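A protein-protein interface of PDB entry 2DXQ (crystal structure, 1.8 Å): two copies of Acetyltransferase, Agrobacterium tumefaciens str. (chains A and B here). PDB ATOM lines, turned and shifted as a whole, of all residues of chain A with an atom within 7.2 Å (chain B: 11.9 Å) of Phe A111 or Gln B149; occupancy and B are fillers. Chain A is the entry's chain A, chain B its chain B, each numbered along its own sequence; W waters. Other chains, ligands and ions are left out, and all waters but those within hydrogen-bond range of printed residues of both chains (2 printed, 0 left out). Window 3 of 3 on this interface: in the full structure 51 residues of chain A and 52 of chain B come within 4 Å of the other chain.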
ATOM      1  N   LEU A  68      -5.050 -14.453 -19.580  1.00  0.00           N
ATOM      2  CA  LEU A  68      -3.860 -14.984 -18.942  1.00  0.00           C
ATOM      3  C   LEU A  68      -2.768 -13.929 -18.972  1.00  0.00           C
ATOM      4  O   LEU A  68      -2.511 -13.333 -20.018  1.00  0.00           O
ATOM      5  CB  LEU A  68      -3.376 -16.232 -19.680  1.00  0.00           C
ATOM      6  CG  LEU A  68      -2.086 -16.879 -19.187  1.00  0.00           C
ATOM      7  CD1 LEU A  68      -2.221 -17.388 -17.736  1.00  0.00           C
ATOM      8  CD2 LEU A  68      -1.740 -18.024 -20.156  1.00  0.00           C
ATOM      9  N   ILE A  70       1.190 -13.732 -18.119  1.00  0.00           N
ATOM     10  CA  ILE A  70       2.423 -14.443 -17.758  1.00  0.00           C
ATOM     11  C   ILE A  70       3.492 -13.395 -17.492  1.00  0.00           C
ATOM     12  O   ILE A  70       3.681 -12.479 -18.301  1.00  0.00           O
ATOM     13  CB  ILE A  70       2.897 -15.409 -18.874  1.00  0.00           C
ATOM     14  CG1 ILE A  70       1.861 -16.524 -19.090  1.00  0.00           C
ATOM     15  CG2 ILE A  70       4.261 -16.020 -18.502  1.00  0.00           C
ATOM     16  CD1 ILE A  70       2.106 -17.383 -20.372  1.00  0.00           C
ATOM     17  N   ARG A  79      11.686 -18.703 -12.654  1.00  0.00           N
ATOM     18  CA  ARG A  79      10.533 -19.200 -13.401  1.00  0.00           C
ATOM     19  C   ARG A  79       9.402 -18.197 -13.350  1.00  0.00           C
ATOM     20  O   ARG A  79       9.180 -17.583 -12.301  1.00  0.00           O
ATOM     21  CB  ARG A  79      10.068 -20.519 -12.822  1.00  0.00           C
ATOM     22  CG  ARG A  79      11.006 -21.669 -13.141  1.00  0.00           C
ATOM     23  CD  ARG A  79      10.517 -22.911 -12.503  1.00  0.00           C
ATOM     24  NE  ARG A  79       9.367 -23.482 -13.202  1.00  0.00           N
ATOM     25  CZ  ARG A  79       8.678 -24.523 -12.748  1.00  0.00           C
ATOM     26  NH1 ARG A  79       9.030 -25.095 -11.598  1.00  0.00           N
ATOM     27  NH2 ARG A  79       7.639 -24.997 -13.438  1.00  0.00           N
ATOM     28  N   ALA A  82       1.952 -16.609 -13.187  1.00  0.00           N
ATOM     29  CA  ALA A  82       0.853 -16.091 -13.984  1.00  0.00           C
ATOM     30  C   ALA A  82      -0.334 -15.720 -13.126  1.00  0.00           C
ATOM     31  O   ALA A  82      -0.513 -16.272 -12.036  1.00  0.00           O
ATOM     32  CB  ALA A  82       0.431 -17.124 -15.024  1.00  0.00           C
ATOM     33  N   HIS A 105      -7.744 -24.057 -19.947  1.00  0.00           N
ATOM     34  CA  HIS A 105      -6.823 -23.816 -21.061  1.00  0.00           C
ATOM     35  C   HIS A 105      -5.770 -22.776 -20.695  1.00  0.00           C
ATOM     36  O   HIS A 105      -4.580 -22.952 -20.965  1.00  0.00           O
ATOM     37  CB  HIS A 105      -7.552 -23.396 -22.335  1.00  0.00           C
ATOM     38  CG  HIS A 105      -6.650 -23.261 -23.521  1.00  0.00           C
ATOM     39  ND1 HIS A 105      -6.171 -24.348 -24.223  1.00  0.00           N
ATOM     40  CD2 HIS A 105      -6.150 -22.162 -24.139  1.00  0.00           C
ATOM     41  CE1 HIS A 105      -5.408 -23.923 -25.219  1.00  0.00           C
ATOM     42  NE2 HIS A 105      -5.380 -22.600 -25.192  1.00  0.00           N
ATOM     43  N   ALA A 106      -6.209 -21.707 -20.045  1.00  0.00           N
ATOM     44  CA  ALA A 106      -5.295 -20.669 -19.591  1.00  0.00           C
ATOM     45  C   ALA A 106      -4.276 -21.216 -18.571  1.00  0.00           C
ATOM     46  O   ALA A 106      -3.072 -20.929 -18.670  1.00  0.00           O
ATOM     47  CB  ALA A 106      -6.109 -19.472 -19.030  1.00  0.00           C
ATOM     48  N   ILE A 107      -4.737 -22.050 -17.637  1.00  0.00           N
ATOM     49  CA  ILE A 107      -3.839 -22.721 -16.678  1.00  0.00           C
ATOM     50  C   ILE A 107      -2.815 -23.562 -17.435  1.00  0.00           C
ATOM     51  O   ILE A 107      -1.607 -23.470 -17.200  1.00  0.00           O
ATOM     52  CB  ILE A 107      -4.623 -23.591 -15.698  1.00  0.00           C
ATOM     53  CG1 ILE A 107      -5.405 -22.679 -14.742  1.00  0.00           C
ATOM     54  CG2 ILE A 107      -3.673 -24.503 -14.883  1.00  0.00           C
ATOM     55  CD1 ILE A 107      -6.495 -23.395 -13.941  1.00  0.00           C
ATOM     56  N   GLU A 108      -3.313 -24.359 -18.375  1.00  0.00           N
ATOM     57  CA  GLU A 108      -2.432 -25.272 -19.097  1.00  0.00           C
ATOM     58  C   GLU A 108      -1.411 -24.511 -19.921  1.00  0.00           C
ATOM     59  O   GLU A 108      -0.236 -24.907 -19.989  1.00  0.00           O
ATOM     60  CB  GLU A 108      -3.271 -26.244 -19.931  1.00  0.00           C
ATOM     61  CG  GLU A 108      -3.969 -27.244 -19.030  1.00  0.00           C
ATOM     62  CD  GLU A 108      -5.025 -28.084 -19.729  1.00  0.00           C
ATOM     63  OE1 GLU A 108      -5.167 -27.997 -20.972  1.00  0.00           O
ATOM     64  OE2 GLU A 108      -5.719 -28.837 -19.010  1.00  0.00           O
ATOM     65  N   THR A 109      -1.842 -23.388 -20.484  1.00  0.00           N
ATOM     66  CA  THR A 109      -0.958 -22.528 -21.282  1.00  0.00           C
ATOM     67  C   THR A 109       0.153 -21.922 -20.432  1.00  0.00           C
ATOM     68  O   THR A 109       1.329 -21.892 -20.846  1.00  0.00           O
ATOM     69  CB  THR A 109      -1.759 -21.463 -22.040  1.00  0.00           C
ATOM     70  OG1 THR A 109      -2.677 -22.119 -22.925  1.00  0.00           O
ATOM     71  CG2 THR A 109      -0.839 -20.511 -22.851  1.00  0.00           C
ATOM     72  N   ALA A 110      -0.207 -21.483 -19.233  1.00  0.00           N
ATOM     73  CA  ALA A 110       0.769 -20.961 -18.276  1.00  0.00           C
ATOM     74  C   ALA A 110       1.805 -22.024 -17.888  1.00  0.00           C
ATOM     75  O   ALA A 110       3.018 -21.773 -17.903  1.00  0.00           O
ATOM     76  CB  ALA A 110       0.037 -20.458 -17.042  1.00  0.00           C
ATOM     77  N   PHE A 111       1.333 -23.212 -17.534  1.00  0.00           N
ATOM     78  CA  PHE A 111       2.251 -24.295 -17.170  1.00  0.00           C
ATOM     79  C   PHE A 111       3.144 -24.714 -18.343  1.00  0.00           C
ATOM     80  O   PHE A 111       4.332 -25.012 -18.150  1.00  0.00           O
ATOM     81  CB  PHE A 111       1.512 -25.493 -16.592  1.00  0.00           C
ATOM     82  CG  PHE A 111       0.983 -25.273 -15.181  1.00  0.00           C
ATOM     83  CD1 PHE A 111       1.601 -24.378 -14.312  1.00  0.00           C
ATOM     84  CD2 PHE A 111      -0.119 -25.990 -14.731  1.00  0.00           C
ATOM     85  CE1 PHE A 111       1.117 -24.183 -13.012  1.00  0.00           C
ATOM     86  CE2 PHE A 111      -0.611 -25.808 -13.431  1.00  0.00           C
ATOM     87  CZ  PHE A 111       0.007 -24.902 -12.576  1.00  0.00           C
ATOM     88  N   GLY A 112       2.589 -24.694 -19.552  1.00  0.00           N
ATOM     89  CA  GLY A 112       3.400 -24.961 -20.766  1.00  0.00           C
ATOM     90  C   GLY A 112       4.507 -23.932 -20.978  1.00  0.00           C
ATOM     91  O   GLY A 112       5.542 -24.219 -21.610  1.00  0.00           O
ATOM     92  N   ALA A 113       4.291 -22.727 -20.449  1.00  0.00           N
ATOM     93  CA  ALA A 113       5.262 -21.621 -20.519  1.00  0.00           C
ATOM     94  C   ALA A 113       6.235 -21.634 -19.330  1.00  0.00           C
ATOM     95  O   ALA A 113       7.010 -20.679 -19.136  1.00  0.00           O
ATOM     96  CB  ALA A 113       4.516 -20.275 -20.583  1.00  0.00           C
ATOM     97  N   ASN A 114       6.175 -22.721 -18.561  1.00  0.00           N
ATOM     98  CA  ASN A 114       7.019 -23.008 -17.389  1.00  0.00           C
ATOM     99  C   ASN A 114       6.702 -22.138 -16.174  1.00  0.00           C
ATOM    100  O   ASN A 114       7.563 -21.933 -15.330  1.00  0.00           O
ATOM    101  CB  ASN A 114       8.531 -22.938 -17.703  1.00  0.00           C
ATOM    102  CG  ASN A 114       9.374 -23.715 -16.694  1.00  0.00           C
ATOM    103  OD1 ASN A 114       8.936 -24.720 -16.139  1.00  0.00           O
ATOM    104  ND2 ASN A 114      10.592 -23.236 -16.446  1.00  0.00           N
ATOM    105  N   CYS A 115       5.467 -21.648 -16.075  1.00  0.00           N
ATOM    106  CA  CYS A 115       5.068 -20.931 -14.851  1.00  0.00           C
ATOM    107  C   CYS A 115       5.022 -21.891 -13.663  1.00  0.00           C
ATOM    108  O   CYS A 115       4.477 -22.996 -13.765  1.00  0.00           O
ATOM    109  CB  CYS A 115       3.697 -20.259 -15.022  1.00  0.00           C
ATOM    110  SG  CYS A 115       3.676 -18.885 -16.132  1.00  0.00           S
ATOM    111  N   TYR A 116       5.586 -21.488 -12.525  1.00  0.00           N
ATOM    112  CA  TYR A 116       5.542 -22.361 -11.354  1.00  0.00           C
ATOM    113  C   TYR A 116       4.213 -22.312 -10.604  1.00  0.00           C
ATOM    114  O   TYR A 116       3.859 -23.238  -9.871  1.00  0.00           O
ATOM    115  CB  TYR A 116       6.736 -22.118 -10.429  1.00  0.00           C
ATOM    116  CG  TYR A 116       6.688 -20.864  -9.592  1.00  0.00           C
ATOM    117  CD1 TYR A 116       7.215 -19.669 -10.065  1.00  0.00           C
ATOM    118  CD2 TYR A 116       6.161 -20.893  -8.301  1.00  0.00           C
ATOM    119  CE1 TYR A 116       7.198 -18.520  -9.282  1.00  0.00           C
ATOM    120  CE2 TYR A 116       6.135 -19.742  -7.522  1.00  0.00           C
ATOM    121  CZ  TYR A 116       6.657 -18.567  -8.019  1.00  0.00           C
ATOM    122  OH  TYR A 116       6.650 -17.422  -7.241  1.00  0.00           O
ATOM    123  N   LYS A 117       3.480 -21.217 -10.780  1.00  0.00           N
ATOM    124  CA  LYS A 117       2.172 -21.082 -10.164  1.00  0.00           C
ATOM    125  C   LYS A 117       1.272 -20.215 -11.039  1.00  0.00           C
ATOM    126  O   LYS A 117       1.750 -19.417 -11.860  1.00  0.00           O
ATOM    127  CB  LYS A 117       2.283 -20.475  -8.760  1.00  0.00           C
ATOM    128  CG  LYS A 117       2.710 -19.021  -8.763  1.00  0.00           C
ATOM    129  CD  LYS A 117       2.797 -18.444  -7.344  1.00  0.00           C
ATOM    130  CE  LYS A 117       3.525 -17.111  -7.393  1.00  0.00           C
ATOM    131  NZ  LYS A 117       3.521 -16.427  -6.055  1.00  0.00           N
ATOM    132  N   VAL A 118      -0.028 -20.410 -10.884  1.00  0.00           N
ATOM    133  CA  VAL A 118      -1.026 -19.548 -11.506  1.00  0.00           C
ATOM    134  C   VAL A 118      -1.944 -19.055 -10.387  1.00  0.00           C
ATOM    135  O   VAL A 118      -2.426 -19.859  -9.606  1.00  0.00           O
ATOM    136  CB  VAL A 118      -1.843 -20.304 -12.585  1.00  0.00           C
ATOM    137  CG1 VAL A 118      -2.855 -19.356 -13.248  1.00  0.00           C
ATOM    138  CG2 VAL A 118      -0.904 -20.879 -13.647  1.00  0.00           C
ATOM    139  N   ASP B  30      15.179 -21.084  -2.153  1.00  0.00           N
ATOM    140  CA  ASP B  30      15.467 -20.943  -3.590  1.00  0.00           C
ATOM    141  C   ASP B  30      16.934 -21.164  -3.964  1.00  0.00           C
ATOM    142  O   ASP B  30      17.831 -20.660  -3.282  1.00  0.00           O
ATOM    143  CB  ASP B  30      15.024 -19.575  -4.119  1.00  0.00           C
ATOM    144  CG  ASP B  30      13.549 -19.524  -4.456  1.00  0.00           C
ATOM    145  OD1 ASP B  30      12.886 -20.581  -4.416  1.00  0.00           O
ATOM    146  OD2 ASP B  30      13.052 -18.415  -4.753  1.00  0.00           O
ATOM    147  N   PHE B 145      -6.925 -17.703  -4.971  1.00  0.00           N
ATOM    148  CA  PHE B 145      -6.786 -19.088  -5.461  1.00  0.00           C
ATOM    149  C   PHE B 145      -5.430 -19.272  -6.117  1.00  0.00           C
ATOM    150  O   PHE B 145      -4.891 -18.338  -6.717  1.00  0.00           O
ATOM    151  CB  PHE B 145      -7.891 -19.406  -6.484  1.00  0.00           C
ATOM    152  CG  PHE B 145      -9.267 -19.493  -5.887  1.00  0.00           C
ATOM    153  CD1 PHE B 145      -9.794 -20.727  -5.494  1.00  0.00           C
ATOM    154  CD2 PHE B 145     -10.046 -18.355  -5.741  1.00  0.00           C
ATOM    155  CE1 PHE B 145     -11.077 -20.813  -4.932  1.00  0.00           C
ATOM    156  CE2 PHE B 145     -11.333 -18.427  -5.186  1.00  0.00           C
ATOM    157  CZ  PHE B 145     -11.848 -19.658  -4.779  1.00  0.00           C
ATOM    158  N   GLN B 146      -4.879 -20.480  -6.037  1.00  0.00           N
ATOM    159  CA  GLN B 146      -3.605 -20.733  -6.674  1.00  0.00           C
ATOM    160  C   GLN B 146      -3.513 -22.181  -7.085  1.00  0.00           C
ATOM    161  O   GLN B 146      -4.104 -23.042  -6.456  1.00  0.00           O
ATOM    162  CB  GLN B 146      -2.464 -20.385  -5.700  1.00  0.00           C
ATOM    163  CG  GLN B 146      -1.070 -20.521  -6.268  1.00  0.00           C
ATOM    164  CD  GLN B 146      -0.041 -19.827  -5.404  1.00  0.00           C
ATOM    165  OE1 GLN B 146      -0.089 -18.603  -5.216  1.00  0.00           O
ATOM    166  NE2 GLN B 146       0.880 -20.591  -4.861  1.00  0.00           N
ATOM    167  N   ILE B 147      -2.777 -22.426  -8.157  1.00  0.00           N
ATOM    168  CA  ILE B 147      -2.420 -23.793  -8.543  1.00  0.00           C
ATOM    169  C   ILE B 147      -0.937 -23.774  -8.864  1.00  0.00           C
ATOM    170  O   ILE B 147      -0.423 -22.807  -9.415  1.00  0.00           O
ATOM    171  CB  ILE B 147      -3.292 -24.320  -9.719  1.00  0.00           C
ATOM    172  CG1 ILE B 147      -2.977 -25.798 -10.037  1.00  0.00           C
ATOM    173  CG2 ILE B 147      -3.157 -23.441 -10.964  1.00  0.00           C
ATOM    174  CD1 ILE B 147      -3.936 -26.396 -11.101  1.00  0.00           C
ATOM    175  N   ARG B 148      -0.248 -24.846  -8.495  1.00  0.00           N
ATOM    176  CA  ARG B 148       1.197 -24.911  -8.647  1.00  0.00           C
ATOM    177  C   ARG B 148       1.604 -26.135  -9.464  1.00  0.00           C
ATOM    178  O   ARG B 148       0.851 -27.108  -9.554  1.00  0.00           O
ATOM    179  CB  ARG B 148       1.867 -24.944  -7.273  1.00  0.00           C
ATOM    180  CG  ARG B 148       1.626 -23.697  -6.421  1.00  0.00           C
ATOM    181  CD  ARG B 148       2.297 -23.785  -5.045  1.00  0.00           C
ATOM    182  NE  ARG B 148       3.742 -23.583  -5.123  1.00  0.00           N
ATOM    183  CZ  ARG B 148       4.360 -22.418  -4.930  1.00  0.00           C
ATOM    184  NH1 ARG B 148       3.671 -21.322  -4.635  1.00  0.00           N
ATOM    185  NH2 ARG B 148       5.682 -22.346  -5.030  1.00  0.00           N
ATOM    186  N   GLN B 149       2.788 -26.074 -10.065  1.00  0.00           N
ATOM    187  CA  GLN B 149       3.396 -27.271 -10.638  1.00  0.00           C
ATOM    188  C   GLN B 149       4.817 -27.473 -10.102  1.00  0.00           C
ATOM    189  O   GLN B 149       5.560 -26.502  -9.900  1.00  0.00           O
ATOM    190  CB  GLN B 149       3.366 -27.242 -12.174  1.00  0.00           C
ATOM    191  CG  GLN B 149       4.261 -26.201 -12.847  1.00  0.00           C
ATOM    192  CD  GLN B 149       4.389 -26.431 -14.354  1.00  0.00           C
ATOM    193  OE1 GLN B 149       4.085 -27.522 -14.858  1.00  0.00           O
ATOM    194  NE2 GLN B 149       4.847 -25.411 -15.075  1.00  0.00           N
HETATM  195  O   HOH W   1       1.383 -16.644  -3.931  1.00  0.00           O
HETATM  196  O   HOH W   2       7.744 -28.178 -10.628  1.00  0.00           O
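The guanidinium group (NH2) of Arg A79 sits close to the side-chain amide nitrogen (NE2) of Gln B149 (3.3 Å).
The side-chain amide nitrogen (NE2) of Gln B149 sits at hydrogen-bond distance from the backbone carbonyl oxygen (O) of Phe A111.
The backbone carbonyl oxygen (O) of Cys A115 sits at hydrogen-bond distance from the side-chain amide nitrogen (NE2) of Gln B149.
The backbone NH of Gln B149 sits at hydrogen-bond distance from the backbone carbonyl oxygen of Tyr A116 (3.0 Å).
N of Val A118 sits at hydrogen-bond distance from O of Ile B147, 2.8 Å away.
OD1 of Asn A114 lies within hydrogen-bond range of NH2 of Arg A79 (3.0 Å).
N of Ala A82 is in hydrogen-bond range of O of Lys A117 (3.1 Å).
The backbone carbonyl oxygen (O) of Ala A110 lies within hydrogen-bond range of the backbone NH (N) of Cys A115.
The side-chain amino group of Lys A117 lies close to the side-chain hydroxyl of Tyr A116.
The guanidinium group (NH1) of Arg B148 lies close to the side-chain amide nitrogen (NE2) of Gln B146 (2.9 Å).
Ile B147 touches Phe A111 (O to CZ, 3.8 Å).
C of Arg B148 touches CZ of Phe A111, 3.7 Å away.
Asn A114 touches Gln B149 (C to NE2, 3.9 Å).
Tyr A116 touches Arg B148.
Gln B146 touches Lys A117 (OE1 to CD, 3.6 Å).
CA of Lys A117 touches O of Ile B147, 3.2 Å away.
CA of Gln B146 touches O of Val A118 (3.3 Å).
No residue of chain B comes within 4 Å of Ala A110.
Of chain B, only Ile B147, Arg B148 and Gln B149 come within 4 Å of Phe A111.
No residue of chain B comes within 4 Å of Gly A112.
Ala A113 touches none of the printed residues of chain B.
Of chain B, only Gln B149 (3.9 Å) comes within 4 Å of Asn A114.
Cys A115 touches just one residue of chain B: Gln B149 (2.8 Å).
Printed residues of chain B within 4 Å of Val A118: Gln B146 (3.3 Å) and Ile B147 (2.8 Å).
Asp B30 touches none of the printed residues of chain A.
Of the printed residues of chain A, Gln B146 touches Lys A117 (3.6 Å) and Val A118 (3.3 Å).
Printed residues of chain A within 4 Å of Arg B148: Phe A111 and Tyr A116.
Of chain A, only Arg A79, Phe A111, Asn A114, Cys A115 and Tyr A116 come within 4 Å of Gln B149.
Of the 18 printed residues of chain A, 7 touch a printed residue of chain B.
Hydrophobic or aromatic side chains of chain A within 4 Å of the printed part of chain B: Phe A111, Tyr A116 and Val A118.
Hydrophobic or aromatic side chains of chain B that line the printed part of chain A: Ile B147.
Among the printed residues, 12 pairs touch across the chains.
Among the printed residues, no Asp or Glu carboxylate lies within 4 Å of a Lys or Arg side-chain nitrogen of the other chain.
No position is printed for both chains.
Water W1 lies within hydrogen-bond range of the side-chain amide oxygen of Gln B146 (2.8 Å) and the side-chain amino group of Lys A117 (3.0 Å).
Water W2 bridges O of Gln B149 and NH1 of Arg A79.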
